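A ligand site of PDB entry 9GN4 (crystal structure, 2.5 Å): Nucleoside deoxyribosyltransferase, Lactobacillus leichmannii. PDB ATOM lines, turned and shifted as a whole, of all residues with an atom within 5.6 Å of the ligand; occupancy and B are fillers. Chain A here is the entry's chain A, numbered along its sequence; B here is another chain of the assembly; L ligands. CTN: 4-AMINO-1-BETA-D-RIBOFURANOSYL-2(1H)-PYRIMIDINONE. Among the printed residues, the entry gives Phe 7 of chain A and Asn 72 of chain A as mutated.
O3' of the ligand lies within hydrogen-bond range of N of Ala 10 (3.2 Å). OE1 of Gln 46 sits close to N3 of the ligand (3.3 Å). OD2 of Asp 92 is in hydrogen-bond range of O5' of the ligand (2.5 Å). The side-chain carboxylate (OE1) of Glu 98 lies within hydrogen-bond range of an oxygen (O2') of the ligand, 2.6 Å away. The chain-end carboxylate of Tyr 157 of chain B sits at hydrogen-bond distance from a nitrogen (N4) of the ligand (3.0 Å). ND2 of Asn 123 of chain B sits at hydrogen-bond distance from O5' of the ligand, 3.0 Å away. O2' of the ligand sits at hydrogen-bond distance from OD1 of Asn 72, at 2.8 Å.
The side-chain amide nitrogen (ND2) of Asn 123 of chain B lies within hydrogen-bond range of the side-chain hydroxyl (OH) of Tyr 157 of chain B (3.4 Å). N of Gly 94 is in hydrogen-bond range of OD2 of Asp 92 (3.2 Å). O of Pro 42 sits close to OE1 of Gln 46, at 3.0 Å. The side-chain hydroxyl of Thr 68 lies within hydrogen-bond range of the backbone carbonyl oxygen of Trp 64 (2.8 Å). The backbone NH (N) of Leu 95 sits at hydrogen-bond distance from the side-chain carboxylate (OD2) of Asp 92 (2.9 Å). N of Met 125 of chain B is in hydrogen-bond range of OD1 of Asn 123 of chain B (2.8 Å). ND2 of Asn 72 is in hydrogen-bond range of O of Thr 68 (2.9 Å). The chain-end carboxylate of Tyr 157 of chain B sits at hydrogen-bond distance from the backbone NH of Leu 124 of chain B.
CZ of Phe 7 touches O2' of the ligand, at 3.3 Å. Gly 9 touches the ligand (CA to O3', 3.6 Å). Trp 12 touches the ligand. Phe 13 touches the ligand. Pro 42 touches the ligand. Trp 64 touches the ligand. Gly 94 touches the ligand (CA to O5', 3.6 Å). Leu 124 of chain B touches the ligand (CB to C5, 3.8 Å). CG of Met 125 of chain B touches O4' of the ligand (3.3 Å). Hydrophobic or aromatic side chains within 4 Å of the ligand: Phe 7, Trp 12, Phe 13, Pro 42, Trp 64, Leu 124 of chain B and Met 125 of chain B. Of the 23 residues printed, 16 come within 4 Å of the ligand. Along chain A the residues within 4 Å of the ligand span positions 7 to 98. The nearest printed residue that does not touch the ligand is Leu 95 (4.1 Å).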
ATOM      1  N   PHE A   7      -5.798  14.017  23.521  1.00  0.00           N
ATOM      2  CA  PHE A   7      -6.930  14.920  23.563  1.00  0.00           C
ATOM      3  C   PHE A   7      -8.126  14.171  22.999  1.00  0.00           C
ATOM      4  O   PHE A   7      -8.042  13.598  21.906  1.00  0.00           O
ATOM      5  CB  PHE A   7      -6.539  16.162  22.763  1.00  0.00           C
ATOM      6  CG  PHE A   7      -7.667  17.173  22.622  1.00  0.00           C
ATOM      7  CD1 PHE A   7      -8.623  17.028  21.634  1.00  0.00           C
ATOM      8  CD2 PHE A   7      -7.789  18.239  23.522  1.00  0.00           C
ATOM      9  CE1 PHE A   7      -9.671  17.920  21.539  1.00  0.00           C
ATOM     10  CE2 PHE A   7      -8.815  19.152  23.393  1.00  0.00           C
ATOM     11  CZ  PHE A   7      -9.748  18.991  22.395  1.00  0.00           C
ATOM     12  N   PHE A   8      -9.230  14.172  23.749  1.00  0.00           N
ATOM     13  CA  PHE A   8     -10.414  13.433  23.313  1.00  0.00           C
ATOM     14  C   PHE A   8     -11.291  14.313  22.424  1.00  0.00           C
ATOM     15  O   PHE A   8     -12.233  14.925  22.902  1.00  0.00           O
ATOM     16  CB  PHE A   8     -11.152  12.938  24.555  1.00  0.00           C
ATOM     17  CG  PHE A   8     -12.213  11.890  24.268  1.00  0.00           C
ATOM     18  CD1 PHE A   8     -11.850  10.566  24.083  1.00  0.00           C
ATOM     19  CD2 PHE A   8     -13.568  12.241  24.190  1.00  0.00           C
ATOM     20  CE1 PHE A   8     -12.815   9.619  23.801  1.00  0.00           C
ATOM     21  CE2 PHE A   8     -14.517  11.302  23.903  1.00  0.00           C
ATOM     22  CZ  PHE A   8     -14.144   9.985  23.724  1.00  0.00           C
ATOM     23  N   GLY A   9     -10.988  14.329  21.118  1.00  0.00           N
ATOM     24  CA  GLY A   9     -11.807  15.069  20.164  1.00  0.00           C
ATOM     25  C   GLY A   9     -13.077  14.287  19.808  1.00  0.00           C
ATOM     26  O   GLY A   9     -12.997  13.192  19.273  1.00  0.00           O
ATOM     27  N   ALA A  10     -14.226  14.877  20.054  1.00  0.00           N
ATOM     28  CA  ALA A  10     -15.508  14.215  19.828  1.00  0.00           C
ATOM     29  C   ALA A  10     -16.642  15.201  20.027  1.00  0.00           C
ATOM     30  O   ALA A  10     -16.672  15.864  21.059  1.00  0.00           O
ATOM     31  CB  ALA A  10     -15.706  13.077  20.822  1.00  0.00           C
ATOM     32  N   GLY A  11     -17.620  15.184  19.121  1.00  0.00           N
ATOM     33  CA  GLY A  11     -18.918  15.812  19.343  1.00  0.00           C
ATOM     34  C   GLY A  11     -19.775  15.074  20.367  1.00  0.00           C
ATOM     35  O   GLY A  11     -19.586  13.873  20.634  1.00  0.00           O
ATOM     36  N   TRP A  12     -20.757  15.817  20.940  1.00  0.00           N
ATOM     37  CA  TRP A  12     -21.710  15.200  21.856  1.00  0.00           C
ATOM     38  C   TRP A  12     -23.127  15.715  21.598  1.00  0.00           C
ATOM     39  O   TRP A  12     -23.913  15.821  22.545  1.00  0.00           O
ATOM     40  CB  TRP A  12     -21.264  15.401  23.312  1.00  0.00           C
ATOM     41  CG  TRP A  12     -20.985  16.825  23.704  1.00  0.00           C
ATOM     42  CD1 TRP A  12     -21.923  17.754  24.059  1.00  0.00           C
ATOM     43  CD2 TRP A  12     -19.701  17.487  23.853  1.00  0.00           C
ATOM     44  NE1 TRP A  12     -21.316  18.932  24.400  1.00  0.00           N
ATOM     45  CE2 TRP A  12     -19.963  18.806  24.285  1.00  0.00           C
ATOM     46  CE3 TRP A  12     -18.379  17.101  23.638  1.00  0.00           C
ATOM     47  CZ2 TRP A  12     -18.936  19.734  24.519  1.00  0.00           C
ATOM     48  CZ3 TRP A  12     -17.362  18.013  23.856  1.00  0.00           C
ATOM     49  CH2 TRP A  12     -17.634  19.296  24.337  1.00  0.00           C
ATOM     50  N   PHE A  13     -23.449  15.908  20.300  1.00  0.00           N
ATOM     51  CA  PHE A  13     -24.588  16.706  19.849  1.00  0.00           C
ATOM     52  C   PHE A  13     -25.648  15.886  19.115  1.00  0.00           C
ATOM     53  O   PHE A  13     -26.599  16.489  18.626  1.00  0.00           O
ATOM     54  CB  PHE A  13     -24.144  17.814  18.871  1.00  0.00           C
ATOM     55  CG  PHE A  13     -22.977  18.634  19.423  1.00  0.00           C
ATOM     56  CD1 PHE A  13     -23.121  19.398  20.593  1.00  0.00           C
ATOM     57  CD2 PHE A  13     -21.744  18.642  18.768  1.00  0.00           C
ATOM     58  CE1 PHE A  13     -22.040  20.063  21.133  1.00  0.00           C
ATOM     59  CE2 PHE A  13     -20.679  19.345  19.290  1.00  0.00           C
ATOM     60  CZ  PHE A  13     -20.827  20.044  20.479  1.00  0.00           C
ATOM     61  N   PRO A  42     -12.560  17.263  26.860  1.00  0.00           N
ATOM     62  CA  PRO A  42     -13.203  18.574  26.802  1.00  0.00           C
ATOM     63  C   PRO A  42     -14.423  18.735  27.712  1.00  0.00           C
ATOM     64  O   PRO A  42     -14.587  19.762  28.359  1.00  0.00           O
ATOM     65  CB  PRO A  42     -13.581  18.709  25.343  1.00  0.00           C
ATOM     66  CG  PRO A  42     -12.527  17.885  24.635  1.00  0.00           C
ATOM     67  CD  PRO A  42     -12.288  16.688  25.535  1.00  0.00           C
ATOM     68  N   LEU A  43     -15.266  17.708  27.805  1.00  0.00           N
ATOM     69  CA  LEU A  43     -16.510  17.836  28.548  1.00  0.00           C
ATOM     70  C   LEU A  43     -16.241  17.979  30.051  1.00  0.00           C
ATOM     71  O   LEU A  43     -17.056  18.565  30.733  1.00  0.00           O
ATOM     72  CB  LEU A  43     -17.399  16.654  28.195  1.00  0.00           C
ATOM     73  CG  LEU A  43     -18.910  16.859  28.161  1.00  0.00           C
ATOM     74  CD1 LEU A  43     -19.429  18.160  27.585  1.00  0.00           C
ATOM     75  CD2 LEU A  43     -19.429  15.685  27.341  1.00  0.00           C
ATOM     76  N   GLN A  46     -14.858  22.292  30.844  1.00  0.00           N
ATOM     77  CA  GLN A  46     -15.614  23.468  30.452  1.00  0.00           C
ATOM     78  C   GLN A  46     -15.367  24.502  31.548  1.00  0.00           C
ATOM     79  O   GLN A  46     -15.214  24.159  32.718  1.00  0.00           O
ATOM     80  CB  GLN A  46     -17.119  23.223  30.286  1.00  0.00           C
ATOM     81  CG  GLN A  46     -17.513  22.051  29.393  1.00  0.00           C
ATOM     82  CD  GLN A  46     -17.375  22.338  27.906  1.00  0.00           C
ATOM     83  OE1 GLN A  46     -16.427  21.885  27.247  1.00  0.00           O
ATOM     84  NE2 GLN A  46     -18.280  23.134  27.367  1.00  0.00           N
ATOM     85  N   VAL A  52     -22.964  24.596  28.454  1.00  0.00           N
ATOM     86  CA  VAL A  52     -23.851  25.637  27.985  1.00  0.00           C
ATOM     87  C   VAL A  52     -25.251  25.073  27.706  1.00  0.00           C
ATOM     88  O   VAL A  52     -26.192  25.839  27.669  1.00  0.00           O
ATOM     89  CB  VAL A  52     -23.266  26.383  26.766  1.00  0.00           C
ATOM     90  CG1 VAL A  52     -23.329  25.560  25.486  1.00  0.00           C
ATOM     91  CG2 VAL A  52     -23.907  27.747  26.544  1.00  0.00           C
ATOM     92  N   TRP A  64     -16.705  32.878  29.337  1.00  0.00           N
ATOM     93  CA  TRP A  64     -16.850  31.428  29.351  1.00  0.00           C
ATOM     94  C   TRP A  64     -16.311  30.850  28.041  1.00  0.00           C
ATOM     95  O   TRP A  64     -15.580  29.855  28.062  1.00  0.00           O
ATOM     96  CB  TRP A  64     -18.315  31.025  29.587  1.00  0.00           C
ATOM     97  CG  TRP A  64     -18.547  29.538  29.493  1.00  0.00           C
ATOM     98  CD1 TRP A  64     -18.487  28.656  30.516  1.00  0.00           C
ATOM     99  CD2 TRP A  64     -18.805  28.769  28.299  1.00  0.00           C
ATOM    100  NE1 TRP A  64     -18.711  27.384  30.055  1.00  0.00           N
ATOM    101  CE2 TRP A  64     -18.906  27.420  28.702  1.00  0.00           C
ATOM    102  CE3 TRP A  64     -18.986  29.081  26.949  1.00  0.00           C
ATOM    103  CZ2 TRP A  64     -19.148  26.390  27.796  1.00  0.00           C
ATOM    104  CZ3 TRP A  64     -19.239  28.063  26.049  1.00  0.00           C
ATOM    105  CH2 TRP A  64     -19.344  26.733  26.473  1.00  0.00           C
ATOM    106  N   THR A  68     -13.100  28.463  27.681  1.00  0.00           N
ATOM    107  CA  THR A  68     -13.328  27.099  27.216  1.00  0.00           C
ATOM    108  C   THR A  68     -12.546  26.878  25.909  1.00  0.00           C
ATOM    109  O   THR A  68     -11.923  25.819  25.754  1.00  0.00           O
ATOM    110  CB  THR A  68     -14.835  26.819  27.082  1.00  0.00           C
ATOM    111  OG1 THR A  68     -15.451  27.114  28.325  1.00  0.00           O
ATOM    112  CG2 THR A  68     -15.131  25.362  26.803  1.00  0.00           C
ATOM    113  N   ASN A  72      -9.297  24.170  25.481  1.00  0.00           N
ATOM    114  CA  ASN A  72      -9.226  23.143  24.469  1.00  0.00           C
ATOM    115  C   ASN A  72      -7.895  23.213  23.717  1.00  0.00           C
ATOM    116  O   ASN A  72      -7.260  22.183  23.481  1.00  0.00           O
ATOM    117  CB  ASN A  72     -10.394  23.253  23.487  1.00  0.00           C
ATOM    118  CG  ASN A  72     -11.672  22.631  24.017  1.00  0.00           C
ATOM    119  OD1 ASN A  72     -11.753  21.416  24.167  1.00  0.00           O
ATOM    120  ND2 ASN A  72     -12.703  23.427  24.215  1.00  0.00           N
ATOM    121  N   ASP A  92     -18.304  17.097  12.463  1.00  0.00           N
ATOM    122  CA  ASP A  92     -18.367  18.191  13.426  1.00  0.00           C
ATOM    123  C   ASP A  92     -17.346  19.292  13.098  1.00  0.00           C
ATOM    124  O   ASP A  92     -16.126  19.050  13.071  1.00  0.00           O
ATOM    125  CB  ASP A  92     -18.149  17.665  14.832  1.00  0.00           C
ATOM    126  CG  ASP A  92     -18.342  18.711  15.920  1.00  0.00           C
ATOM    127  OD1 ASP A  92     -19.512  19.087  16.173  1.00  0.00           O
ATOM    128  OD2 ASP A  92     -17.328  19.186  16.456  1.00  0.00           O
ATOM    129  N   VAL A  93     -17.856  20.512  12.867  1.00  0.00           N
ATOM    130  CA  VAL A  93     -17.002  21.637  12.494  1.00  0.00           C
ATOM    131  C   VAL A  93     -15.958  21.903  13.592  1.00  0.00           C
ATOM    132  O   VAL A  93     -14.828  22.279  13.296  1.00  0.00           O
ATOM    133  CB  VAL A  93     -17.865  22.886  12.207  1.00  0.00           C
ATOM    134  CG1 VAL A  93     -18.571  23.409  13.448  1.00  0.00           C
ATOM    135  CG2 VAL A  93     -17.059  24.005  11.590  1.00  0.00           C
ATOM    136  N   GLY A  94     -16.351  21.726  14.863  1.00  0.00           N
ATOM    137  CA  GLY A  94     -15.455  22.001  15.991  1.00  0.00           C
ATOM    138  C   GLY A  94     -14.254  21.058  15.969  1.00  0.00           C
ATOM    139  O   GLY A  94     -13.108  21.483  16.114  1.00  0.00           O
ATOM    140  N   LEU A  95     -14.541  19.757  15.820  1.00  0.00           N
ATOM    141  CA  LEU A  95     -13.498  18.759  15.711  1.00  0.00           C
ATOM    142  C   LEU A  95     -12.613  19.089  14.513  1.00  0.00           C
ATOM    143  O   LEU A  95     -11.400  18.980  14.586  1.00  0.00           O
ATOM    144  CB  LEU A  95     -14.101  17.366  15.566  1.00  0.00           C
ATOM    145  CG  LEU A  95     -13.110  16.210  15.417  1.00  0.00           C
ATOM    146  CD1 LEU A  95     -12.086  16.227  16.544  1.00  0.00           C
ATOM    147  CD2 LEU A  95     -13.878  14.914  15.373  1.00  0.00           C
ATOM    148  N   GLU A  98     -10.105  21.658  15.348  1.00  0.00           N
ATOM    149  CA  GLU A  98      -9.125  21.064  16.249  1.00  0.00           C
ATOM    150  C   GLU A  98      -8.120  20.173  15.505  1.00  0.00           C
ATOM    151  O   GLU A  98      -6.962  20.102  15.919  1.00  0.00           O
ATOM    152  CB  GLU A  98      -9.845  20.294  17.349  1.00  0.00           C
ATOM    153  CG  GLU A  98     -10.569  21.224  18.304  1.00  0.00           C
ATOM    154  CD  GLU A  98     -11.433  20.517  19.336  1.00  0.00           C
ATOM    155  OE1 GLU A  98     -11.710  21.142  20.384  1.00  0.00           O
ATOM    156  OE2 GLU A  98     -11.819  19.350  19.067  1.00  0.00           O
ATOM    157  N   ASN B 123     -20.472  26.886  16.659  1.00  0.00           N
ATOM    158  CA  ASN B 123     -19.567  26.084  17.464  1.00  0.00           C
ATOM    159  C   ASN B 123     -18.525  26.954  18.169  1.00  0.00           C
ATOM    160  O   ASN B 123     -17.952  27.856  17.568  1.00  0.00           O
ATOM    161  CB  ASN B 123     -18.879  25.085  16.545  1.00  0.00           C
ATOM    162  CG  ASN B 123     -18.195  24.004  17.349  1.00  0.00           C
ATOM    163  OD1 ASN B 123     -17.143  24.253  17.953  1.00  0.00           O
ATOM    164  ND2 ASN B 123     -18.824  22.844  17.363  1.00  0.00           N
ATOM    165  N   LEU B 124     -18.242  26.641  19.423  1.00  0.00           N
ATOM    166  CA  LEU B 124     -17.220  27.329  20.201  1.00  0.00           C
ATOM    167  C   LEU B 124     -15.924  27.495  19.414  1.00  0.00           C
ATOM    168  O   LEU B 124     -15.332  28.564  19.446  1.00  0.00           O
ATOM    169  CB  LEU B 124     -16.919  26.551  21.485  1.00  0.00           C
ATOM    170  CG  LEU B 124     -15.767  27.095  22.333  1.00  0.00           C
ATOM    171  CD1 LEU B 124     -16.128  28.465  22.863  1.00  0.00           C
ATOM    172  CD2 LEU B 124     -15.424  26.159  23.498  1.00  0.00           C
ATOM    173  N   MET B 125     -15.492  26.421  18.726  1.00  0.00           N
ATOM    174  CA  MET B 125     -14.173  26.408  18.143  1.00  0.00           C
ATOM    175  C   MET B 125     -14.177  27.277  16.893  1.00  0.00           C
ATOM    176  O   MET B 125     -13.164  27.899  16.592  1.00  0.00           O
ATOM    177  CB  MET B 125     -13.708  24.969  17.860  1.00  0.00           C
ATOM    178  CG  MET B 125     -13.803  24.057  19.074  1.00  0.00           C
ATOM    179  SD  MET B 125     -12.982  24.705  20.553  1.00  0.00           S
ATOM    180  CE  MET B 125     -11.230  24.647  20.164  1.00  0.00           C
ATOM    181  N   TYR B 157     -22.479  27.383  20.902  1.00  0.00           N
ATOM    182  CA  TYR B 157     -22.805  26.142  21.588  1.00  0.00           C
ATOM    183  C   TYR B 157     -21.508  25.341  21.871  1.00  0.00           C
ATOM    184  O   TYR B 157     -21.633  24.444  22.717  1.00  0.00           O
ATOM    185  CB  TYR B 157     -23.843  25.370  20.767  1.00  0.00           C
ATOM    186  CG  TYR B 157     -23.315  24.782  19.473  1.00  0.00           C
ATOM    187  CD1 TYR B 157     -22.664  23.561  19.472  1.00  0.00           C
ATOM    188  CD2 TYR B 157     -23.506  25.411  18.249  1.00  0.00           C
ATOM    189  CE1 TYR B 157     -22.202  22.982  18.303  1.00  0.00           C
ATOM    190  CE2 TYR B 157     -23.055  24.847  17.064  1.00  0.00           C
ATOM    191  CZ  TYR B 157     -22.408  23.623  17.094  1.00  0.00           C
ATOM    192  OH  TYR B 157     -21.887  23.098  15.954  1.00  0.00           O
ATOM    193  OXT TYR B 157     -20.414  25.609  21.289  1.00  0.00           O
HETATM  194  O5' CTN L   1     -17.432  20.467  18.611  1.00  0.00           O
HETATM  195  C5' CTN L   1     -16.924  19.609  19.669  1.00  0.00           C
HETATM  196  C4' CTN L   1     -15.411  19.753  19.802  1.00  0.00           C
HETATM  197  O4' CTN L   1     -15.021  21.130  20.123  1.00  0.00           O
HETATM  198  C1' CTN L   1     -14.771  21.252  21.507  1.00  0.00           C
HETATM  199  N1  CTN L   1     -15.959  21.878  22.156  1.00  0.00           N
HETATM  200  C6  CTN L   1     -17.019  22.335  21.412  1.00  0.00           C
HETATM  201  C5  CTN L   1     -18.082  22.939  21.999  1.00  0.00           C
HETATM  202  C4  CTN L   1     -18.067  23.092  23.416  1.00  0.00           C
HETATM  203  N3  CTN L   1     -17.019  22.701  24.156  1.00  0.00           N
HETATM  204  C2  CTN L   1     -15.954  22.109  23.548  1.00  0.00           C
HETATM  205  O2  CTN L   1     -14.993  21.719  24.203  1.00  0.00           O
HETATM  206  N4  CTN L   1     -19.092  23.652  24.041  1.00  0.00           N
HETATM  207  C2' CTN L   1     -14.377  19.855  22.020  1.00  0.00           C
HETATM  208  O2' CTN L   1     -12.981  19.820  22.215  1.00  0.00           O
HETATM  209  C3' CTN L   1     -14.792  18.874  20.901  1.00  0.00           C
HETATM  210  O3' CTN L   1     -13.789  18.044  20.324  1.00  0.00           O
